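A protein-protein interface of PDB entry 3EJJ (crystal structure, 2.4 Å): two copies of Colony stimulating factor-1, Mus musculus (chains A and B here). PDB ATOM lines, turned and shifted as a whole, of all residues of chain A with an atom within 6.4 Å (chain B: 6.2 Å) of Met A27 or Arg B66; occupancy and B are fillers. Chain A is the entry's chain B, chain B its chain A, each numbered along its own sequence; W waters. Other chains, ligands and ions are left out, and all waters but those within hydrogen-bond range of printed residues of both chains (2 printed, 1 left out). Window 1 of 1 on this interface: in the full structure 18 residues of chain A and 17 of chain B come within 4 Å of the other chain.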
ATOM      1  N   ILE A  23      -9.065  20.033 -25.039  1.00  0.00           N
ATOM      2  CA  ILE A  23      -9.585  18.688 -24.996  1.00  0.00           C
ATOM      3  C   ILE A  23     -10.571  18.502 -23.845  1.00  0.00           C
ATOM      4  O   ILE A  23     -11.660  17.950 -24.025  1.00  0.00           O
ATOM      5  CB  ILE A  23      -8.441  17.685 -24.866  1.00  0.00           C
ATOM      6  CG1 ILE A  23      -7.499  17.831 -26.059  1.00  0.00           C
ATOM      7  CG2 ILE A  23      -8.993  16.272 -24.799  1.00  0.00           C
ATOM      8  CD1 ILE A  23      -6.221  17.020 -25.936  1.00  0.00           C
ATOM      9  N   ASP A  24     -10.201  18.968 -22.663  1.00  0.00           N
ATOM     10  CA  ASP A  24     -11.066  18.834 -21.504  1.00  0.00           C
ATOM     11  C   ASP A  24     -12.441  19.455 -21.701  1.00  0.00           C
ATOM     12  O   ASP A  24     -13.390  19.092 -21.009  1.00  0.00           O
ATOM     13  CB  ASP A  24     -10.400  19.442 -20.262  1.00  0.00           C
ATOM     14  CG  ASP A  24      -9.154  18.687 -19.844  1.00  0.00           C
ATOM     15  OD1 ASP A  24      -8.979  17.537 -20.304  1.00  0.00           O
ATOM     16  OD2 ASP A  24      -8.357  19.233 -19.050  1.00  0.00           O
ATOM     17  N   SER A  25     -12.562  20.373 -22.652  1.00  0.00           N
ATOM     18  CA  SER A  25     -13.836  21.035 -22.890  1.00  0.00           C
ATOM     19  C   SER A  25     -14.757  20.394 -23.927  1.00  0.00           C
ATOM     20  O   SER A  25     -15.859  20.891 -24.149  1.00  0.00           O
ATOM     21  CB  SER A  25     -13.596  22.482 -23.302  1.00  0.00           C
ATOM     22  OG  SER A  25     -13.018  22.546 -24.597  1.00  0.00           O
ATOM     23  N   GLN A  26     -14.340  19.296 -24.543  1.00  0.00           N
ATOM     24  CA  GLN A  26     -15.153  18.687 -25.582  1.00  0.00           C
ATOM     25  C   GLN A  26     -16.172  17.666 -25.137  1.00  0.00           C
ATOM     26  O   GLN A  26     -15.887  16.810 -24.300  1.00  0.00           O
ATOM     27  CB  GLN A  26     -14.244  18.074 -26.645  1.00  0.00           C
ATOM     28  CG  GLN A  26     -13.381  19.107 -27.344  1.00  0.00           C
ATOM     29  CD  GLN A  26     -14.210  20.188 -27.999  1.00  0.00           C
ATOM     30  OE1 GLN A  26     -14.981  19.915 -28.911  1.00  0.00           O
ATOM     31  NE2 GLN A  26     -14.066  21.415 -27.532  1.00  0.00           N
ATOM     32  N   MET A  27     -17.371  17.749 -25.709  1.00  0.00           N
ATOM     33  CA  MET A  27     -18.431  16.833 -25.355  1.00  0.00           C
ATOM     34  C   MET A  27     -18.142  15.458 -25.892  1.00  0.00           C
ATOM     35  O   MET A  27     -17.812  15.292 -27.051  1.00  0.00           O
ATOM     36  CB  MET A  27     -19.772  17.324 -25.888  1.00  0.00           C
ATOM     37  CG  MET A  27     -20.989  16.580 -25.309  1.00  0.00           C
ATOM     38  SD  MET A  27     -22.527  17.478 -25.583  1.00  0.00           S
ATOM     39  CE  MET A  27     -22.615  17.497 -27.331  1.00  0.00           C
ATOM     40  N   GLU A  28     -18.261  14.459 -25.034  1.00  0.00           N
ATOM     41  CA  GLU A  28     -18.016  13.102 -25.428  1.00  0.00           C
ATOM     42  C   GLU A  28     -19.219  12.532 -26.121  1.00  0.00           C
ATOM     43  O   GLU A  28     -20.131  12.084 -25.456  1.00  0.00           O
ATOM     44  CB  GLU A  28     -17.715  12.245 -24.204  1.00  0.00           C
ATOM     45  CG  GLU A  28     -17.649  10.751 -24.523  1.00  0.00           C
ATOM     46  CD  GLU A  28     -17.667   9.865 -23.298  1.00  0.00           C
ATOM     47  OE1 GLU A  28     -18.723   9.746 -22.661  1.00  0.00           O
ATOM     48  OE2 GLU A  28     -16.618   9.284 -22.973  1.00  0.00           O
ATOM     49  N   THR A  29     -19.240  12.524 -27.448  1.00  0.00           N
ATOM     50  CA  THR A  29     -20.384  11.956 -28.170  1.00  0.00           C
ATOM     51  C   THR A  29     -19.976  10.808 -29.075  1.00  0.00           C
ATOM     52  O   THR A  29     -18.827  10.400 -29.094  1.00  0.00           O
ATOM     53  CB  THR A  29     -21.071  12.994 -29.057  1.00  0.00           C
ATOM     54  OG1 THR A  29     -20.142  13.476 -30.031  1.00  0.00           O
ATOM     55  CG2 THR A  29     -21.580  14.162 -28.229  1.00  0.00           C
ATOM     56  N   LEU A 111     -12.211  13.320 -30.171  1.00  0.00           N
ATOM     57  CA  LEU A 111     -11.504  12.990 -28.961  1.00  0.00           C
ATOM     58  C   LEU A 111     -10.153  12.470 -29.391  1.00  0.00           C
ATOM     59  O   LEU A 111      -9.117  13.025 -29.021  1.00  0.00           O
ATOM     60  CB  LEU A 111     -12.294  11.947 -28.166  1.00  0.00           C
ATOM     61  CG  LEU A 111     -13.673  12.378 -27.607  1.00  0.00           C
ATOM     62  CD1 LEU A 111     -14.587  12.919 -28.731  1.00  0.00           C
ATOM     63  CD2 LEU A 111     -14.342  11.182 -26.909  1.00  0.00           C
ATOM     64  N   LEU B  22     -20.877  26.570 -23.044  1.00  0.00           N
ATOM     65  CA  LEU B  22     -20.682  25.161 -23.348  1.00  0.00           C
ATOM     66  C   LEU B  22     -20.595  25.066 -24.848  1.00  0.00           C
ATOM     67  O   LEU B  22     -19.640  24.547 -25.409  1.00  0.00           O
ATOM     68  CB  LEU B  22     -21.883  24.362 -22.837  1.00  0.00           C
ATOM     69  CG  LEU B  22     -22.041  22.839 -22.970  1.00  0.00           C
ATOM     70  CD1 LEU B  22     -21.004  22.284 -23.888  1.00  0.00           C
ATOM     71  CD2 LEU B  22     -21.924  22.191 -21.615  1.00  0.00           C
ATOM     72  N   GLN B  26     -17.408  24.206 -28.119  1.00  0.00           N
ATOM     73  CA  GLN B  26     -17.327  22.957 -28.872  1.00  0.00           C
ATOM     74  C   GLN B  26     -16.762  23.187 -30.275  1.00  0.00           C
ATOM     75  O   GLN B  26     -17.085  24.168 -30.933  1.00  0.00           O
ATOM     76  CB  GLN B  26     -18.718  22.338 -28.946  1.00  0.00           C
ATOM     77  CG  GLN B  26     -19.322  22.115 -27.584  1.00  0.00           C
ATOM     78  CD  GLN B  26     -18.407  21.299 -26.703  1.00  0.00           C
ATOM     79  OE1 GLN B  26     -18.084  20.151 -27.014  1.00  0.00           O
ATOM     80  NE2 GLN B  26     -17.968  21.891 -25.604  1.00  0.00           N
ATOM     81  N   ILE B  33     -24.952  12.947 -34.926  1.00  0.00           N
ATOM     82  CA  ILE B  33     -25.177  12.042 -33.801  1.00  0.00           C
ATOM     83  C   ILE B  33     -26.665  11.766 -33.765  1.00  0.00           C
ATOM     84  O   ILE B  33     -27.459  12.550 -34.260  1.00  0.00           O
ATOM     85  CB  ILE B  33     -24.731  12.625 -32.457  1.00  0.00           C
ATOM     86  CG1 ILE B  33     -25.217  14.067 -32.329  1.00  0.00           C
ATOM     87  CG2 ILE B  33     -23.232  12.537 -32.325  1.00  0.00           C
ATOM     88  CD1 ILE B  33     -24.797  14.722 -31.062  1.00  0.00           C
ATOM     89  N   ILE B  61     -29.814  15.672 -22.026  1.00  0.00           N
ATOM     90  CA  ILE B  61     -28.895  16.167 -21.047  1.00  0.00           C
ATOM     91  C   ILE B  61     -28.235  15.020 -20.304  1.00  0.00           C
ATOM     92  O   ILE B  61     -27.046  15.042 -20.039  1.00  0.00           O
ATOM     93  CB  ILE B  61     -29.615  17.074 -20.042  1.00  0.00           C
ATOM     94  CG1 ILE B  61     -30.122  18.323 -20.757  1.00  0.00           C
ATOM     95  CG2 ILE B  61     -28.682  17.437 -18.884  1.00  0.00           C
ATOM     96  CD1 ILE B  61     -30.966  19.244 -19.874  1.00  0.00           C
ATOM     97  N   ASP B  62     -29.018  14.007 -20.000  1.00  0.00           N
ATOM     98  CA  ASP B  62     -28.535  12.867 -19.265  1.00  0.00           C
ATOM     99  C   ASP B  62     -27.679  11.928 -20.095  1.00  0.00           C
ATOM    100  O   ASP B  62     -26.600  11.557 -19.678  1.00  0.00           O
ATOM    101  CB  ASP B  62     -29.735  12.122 -18.667  1.00  0.00           C
ATOM    102  CG  ASP B  62     -29.338  10.977 -17.728  1.00  0.00           C
ATOM    103  OD1 ASP B  62     -28.609  11.204 -16.734  1.00  0.00           O
ATOM    104  OD2 ASP B  62     -29.790   9.848 -17.990  1.00  0.00           O
ATOM    105  N   GLU B  63     -28.128  11.554 -21.275  1.00  0.00           N
ATOM    106  CA  GLU B  63     -27.344  10.616 -22.041  1.00  0.00           C
ATOM    107  C   GLU B  63     -26.428  11.142 -23.110  1.00  0.00           C
ATOM    108  O   GLU B  63     -25.624  10.384 -23.623  1.00  0.00           O
ATOM    109  CB  GLU B  63     -28.246   9.518 -22.624  1.00  0.00           C
ATOM    110  CG  GLU B  63     -29.549   9.988 -23.250  1.00  0.00           C
ATOM    111  CD  GLU B  63     -30.748   9.103 -22.861  1.00  0.00           C
ATOM    112  OE1 GLU B  63     -31.214   9.187 -21.699  1.00  0.00           O
ATOM    113  OE2 GLU B  63     -31.222   8.322 -23.716  1.00  0.00           O
ATOM    114  N   THR B  64     -26.499  12.424 -23.431  1.00  0.00           N
ATOM    115  CA  THR B  64     -25.650  12.942 -24.481  1.00  0.00           C
ATOM    116  C   THR B  64     -24.673  14.030 -24.136  1.00  0.00           C
ATOM    117  O   THR B  64     -23.668  14.188 -24.809  1.00  0.00           O
ATOM    118  CB  THR B  64     -26.474  13.421 -25.666  1.00  0.00           C
ATOM    119  OG1 THR B  64     -26.944  12.291 -26.396  1.00  0.00           O
ATOM    120  CG2 THR B  64     -25.647  14.278 -26.586  1.00  0.00           C
ATOM    121  N   MET B  65     -24.942  14.793 -23.102  1.00  0.00           N
ATOM    122  CA  MET B  65     -24.020  15.848 -22.740  1.00  0.00           C
ATOM    123  C   MET B  65     -22.991  15.343 -21.734  1.00  0.00           C
ATOM    124  O   MET B  65     -23.035  15.679 -20.557  1.00  0.00           O
ATOM    125  CB  MET B  65     -24.807  17.036 -22.184  1.00  0.00           C
ATOM    126  CG  MET B  65     -25.748  17.650 -23.197  1.00  0.00           C
ATOM    127  SD  MET B  65     -26.481  19.137 -22.573  1.00  0.00           S
ATOM    128  CE  MET B  65     -28.046  18.920 -23.210  1.00  0.00           C
ATOM    129  N   ARG B  66     -22.057  14.532 -22.217  1.00  0.00           N
ATOM    130  CA  ARG B  66     -21.008  13.962 -21.379  1.00  0.00           C
ATOM    131  C   ARG B  66     -19.706  14.749 -21.418  1.00  0.00           C
ATOM    132  O   ARG B  66     -19.129  14.968 -22.475  1.00  0.00           O
ATOM    133  CB  ARG B  66     -20.731  12.536 -21.800  1.00  0.00           C
ATOM    134  CG  ARG B  66     -21.986  11.738 -21.873  1.00  0.00           C
ATOM    135  CD  ARG B  66     -21.747  10.269 -21.787  1.00  0.00           C
ATOM    136  NE  ARG B  66     -23.017   9.587 -21.979  1.00  0.00           N
ATOM    137  CZ  ARG B  66     -23.223   8.296 -21.763  1.00  0.00           C
ATOM    138  NH1 ARG B  66     -24.426   7.788 -21.980  1.00  0.00           N
ATOM    139  NH2 ARG B  66     -22.237   7.521 -21.322  1.00  0.00           N
ATOM    140  N   PHE B  67     -19.253  15.179 -20.251  1.00  0.00           N
ATOM    141  CA  PHE B  67     -18.027  15.915 -20.129  1.00  0.00           C
ATOM    142  C   PHE B  67     -17.230  15.255 -19.028  1.00  0.00           C
ATOM    143  O   PHE B  67     -17.779  14.462 -18.272  1.00  0.00           O
ATOM    144  CB  PHE B  67     -18.327  17.355 -19.782  1.00  0.00           C
ATOM    145  CG  PHE B  67     -19.077  18.076 -20.854  1.00  0.00           C
ATOM    146  CD1 PHE B  67     -20.473  18.111 -20.847  1.00  0.00           C
ATOM    147  CD2 PHE B  67     -18.394  18.686 -21.903  1.00  0.00           C
ATOM    148  CE1 PHE B  67     -21.170  18.744 -21.869  1.00  0.00           C
ATOM    149  CE2 PHE B  67     -19.073  19.319 -22.928  1.00  0.00           C
ATOM    150  CZ  PHE B  67     -20.463  19.345 -22.909  1.00  0.00           C
ATOM    151  N   LYS B  68     -15.938  15.551 -18.945  1.00  0.00           N
ATOM    152  CA  LYS B  68     -15.101  14.971 -17.903  1.00  0.00           C
ATOM    153  C   LYS B  68     -15.419  15.617 -16.565  1.00  0.00           C
ATOM    154  O   LYS B  68     -15.559  16.832 -16.475  1.00  0.00           O
ATOM    155  CB  LYS B  68     -13.618  15.153 -18.249  1.00  0.00           C
ATOM    156  CG  LYS B  68     -13.098  14.075 -19.185  1.00  0.00           C
ATOM    157  CD  LYS B  68     -11.657  14.321 -19.622  1.00  0.00           C
ATOM    158  CE  LYS B  68     -11.552  15.460 -20.636  1.00  0.00           C
ATOM    159  NZ  LYS B  68     -10.212  15.506 -21.299  1.00  0.00           N
ATOM    160  N   ASN B  73     -17.781  22.511 -18.056  1.00  0.00           N
ATOM    161  CA  ASN B  73     -18.960  22.144 -18.812  1.00  0.00           C
ATOM    162  C   ASN B  73     -19.699  21.066 -18.077  1.00  0.00           C
ATOM    163  O   ASN B  73     -20.920  20.966 -18.155  1.00  0.00           O
ATOM    164  CB  ASN B  73     -18.598  21.612 -20.196  1.00  0.00           C
ATOM    165  CG  ASN B  73     -18.189  22.701 -21.159  1.00  0.00           C
ATOM    166  OD1 ASN B  73     -18.526  23.866 -20.985  1.00  0.00           O
ATOM    167  ND2 ASN B  73     -17.469  22.311 -22.204  1.00  0.00           N
ATOM    168  N   THR B  77     -23.555  21.304 -17.180  1.00  0.00           N
ATOM    169  CA  THR B  77     -24.519  20.306 -17.593  1.00  0.00           C
ATOM    170  C   THR B  77     -25.264  19.754 -16.382  1.00  0.00           C
ATOM    171  O   THR B  77     -26.433  19.380 -16.466  1.00  0.00           O
ATOM    172  CB  THR B  77     -23.830  19.155 -18.271  1.00  0.00           C
ATOM    173  OG1 THR B  77     -22.956  19.657 -19.277  1.00  0.00           O
ATOM    174  CG2 THR B  77     -24.839  18.244 -18.887  1.00  0.00           C
ATOM    175  N   PRO B 110     -23.594  17.761 -33.262  1.00  0.00           N
ATOM    176  CA  PRO B 110     -23.564  18.072 -31.841  1.00  0.00           C
ATOM    177  C   PRO B 110     -23.925  19.521 -31.541  1.00  0.00           C
ATOM    178  O   PRO B 110     -24.546  19.812 -30.526  1.00  0.00           O
ATOM    179  CB  PRO B 110     -22.133  17.746 -31.467  1.00  0.00           C
ATOM    180  CG  PRO B 110     -21.845  16.549 -32.352  1.00  0.00           C
ATOM    181  CD  PRO B 110     -22.406  16.986 -33.663  1.00  0.00           C
ATOM    182  N   LEU B 111     -23.541  20.438 -32.408  1.00  0.00           N
ATOM    183  CA  LEU B 111     -23.844  21.837 -32.173  1.00  0.00           C
ATOM    184  C   LEU B 111     -25.308  22.118 -32.431  1.00  0.00           C
ATOM    185  O   LEU B 111     -25.878  23.030 -31.856  1.00  0.00           O
ATOM    186  CB  LEU B 111     -22.961  22.735 -33.042  1.00  0.00           C
ATOM    187  CG  LEU B 111     -21.542  22.881 -32.469  1.00  0.00           C
ATOM    188  CD1 LEU B 111     -20.584  23.504 -33.495  1.00  0.00           C
ATOM    189  CD2 LEU B 111     -21.612  23.735 -31.212  1.00  0.00           C
ATOM    190  N   LEU B 113     -27.691  19.808 -31.924  1.00  0.00           N
ATOM    191  CA  LEU B 113     -28.382  19.200 -30.805  1.00  0.00           C
ATOM    192  C   LEU B 113     -28.397  20.180 -29.658  1.00  0.00           C
ATOM    193  O   LEU B 113     -29.425  20.412 -29.021  1.00  0.00           O
ATOM    194  CB  LEU B 113     -27.669  17.928 -30.394  1.00  0.00           C
ATOM    195  CG  LEU B 113     -28.201  17.272 -29.138  1.00  0.00           C
ATOM    196  CD1 LEU B 113     -27.873  15.800 -29.206  1.00  0.00           C
ATOM    197  CD2 LEU B 113     -27.576  17.887 -27.903  1.00  0.00           C
ATOM    198  N   LEU B 114     -27.240  20.768 -29.405  1.00  0.00           N
ATOM    199  CA  LEU B 114     -27.117  21.722 -28.335  1.00  0.00           C
ATOM    200  C   LEU B 114     -27.988  22.948 -28.563  1.00  0.00           C
ATOM    201  O   LEU B 114     -28.446  23.571 -27.611  1.00  0.00           O
ATOM    202  CB  LEU B 114     -25.650  22.121 -28.185  1.00  0.00           C
ATOM    203  CG  LEU B 114     -24.779  21.380 -27.172  1.00  0.00           C
ATOM    204  CD1 LEU B 114     -25.443  20.131 -26.652  1.00  0.00           C
ATOM    205  CD2 LEU B 114     -23.457  21.048 -27.831  1.00  0.00           C
HETATM  206  O   HOH W   1     -20.170   8.617 -19.944  1.00  0.00           O
HETATM  207  O   HOH W   2     -14.714  16.595 -21.847  1.00  0.00           O
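Of chain B, only Gln B26 (2.8 Å), Thr B64 (3.6 Å), Met B65 (3.6 Å), Arg B66 (3.5 Å), Phe B67 (3.5 Å) and Leu B114 (3.7 Å) come within 4 Å of Met A27. Arg B66 touches just these residues of chain A: Met A27 and Glu A28. Printed residues of chain A within 4 Å of Phe B67: Ser A25 (3.8 Å), Gln A26 (3.9 Å) and Met A27 (3.5 Å). Printed residues of chain A within 4 Å of Ile B33: Thr A29. Of the printed residues of chain B, Thr A29 touches Ile B33. Of the printed residues of chain B, Ser A25 touches Gln B26 (2.8 Å), Phe B67 (3.8 Å) and Asn B73 (2.9 Å). The nearest residue of chain A that does not touch Arg B66 is Gln A26 (4.2 Å). The nearest printed residue of chain A that does not touch Asn B73 is Gln A26 (4.9 Å).
The backbone carbonyl oxygen (O) of Ser A25 is in hydrogen-bond range of the side-chain amide nitrogen (ND2) of Asn B73. OE1 of Gln B26 lies within hydrogen-bond range of N of Met A27 (2.8 Å). The side-chain sulfur of Met A27 sits close to the backbone carbonyl oxygen of Thr B64 (3.6 Å). NE2 of Gln B26 sits at hydrogen-bond distance from O of Ser A25 (2.8 Å). The backbone carbonyl oxygen (O) of Arg B66 lies within hydrogen-bond range of the backbone NH (N) of Glu A28 (2.7 Å). The side-chain carboxylate of Asp A24 is in salt-bridge range of the side-chain amino group of Lys B68 (2.6 Å).
Of the 17 printed residues of chain B, 9 touch a printed residue of chain A. Along chain B the printed residues that touch a printed residue of chain A span positions 26 to 114. Among the printed residues, 15 pairs touch across the chains. Among the printed residues, Asp or Glu carboxylates within 4 Å of a Lys or Arg side-chain nitrogen of the other chain: Asp A24 with Lys B68 (2.6 Å).
The side-chain amide nitrogen (NE2) of Gln A26 is in hydrogen-bond range of the side-chain hydroxyl (OG) of Ser A25 (3.3 Å). O of Asn B73 is in hydrogen-bond range of OG1 of Thr B77, 2.7 Å away. The guanidinium group of Arg B66 sits at hydrogen-bond distance from the backbone carbonyl oxygen of Glu B63 (3.2 Å). NE2 of Gln B26 sits close to ND2 of Asn B73, at 3.5 Å. The side-chain amide nitrogen (NE2) of Gln B26 sits at hydrogen-bond distance from the backbone carbonyl oxygen (O) of Leu B22, 3.1 Å away.
Water W1 lies within hydrogen-bond range of NH2 of Arg B66 (2.7 Å) and OE1 of Glu A28 (3.3 Å). Water W2 lies within hydrogen-bond range of the backbone carbonyl oxygen (O) of Gln A26 (2.7 Å), the backbone carbonyl oxygen (O) of Asp A24 (2.9 Å) and the backbone NH (N) of Lys B68 (3.3 Å).
Gln B26 touches its own counterpart, Gln A26. Positions printed for both chains: 26 and 111. Of the 15 pairs that touch across the chains among the printed residues, 1 has its exchanged pair printed and touching as well.
Among the printed residues, merely in contact across the chains: Met A27 with Arg B66, Met A27 with Phe B67, Gln A26 with Gln B26, Met A27 with Met B65, Met A27 with Leu B114, Ser A25 with Phe B67, Ile A23 with Lys B68, Gln A26 with Phe B67 and Thr A29 with Ile B33.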
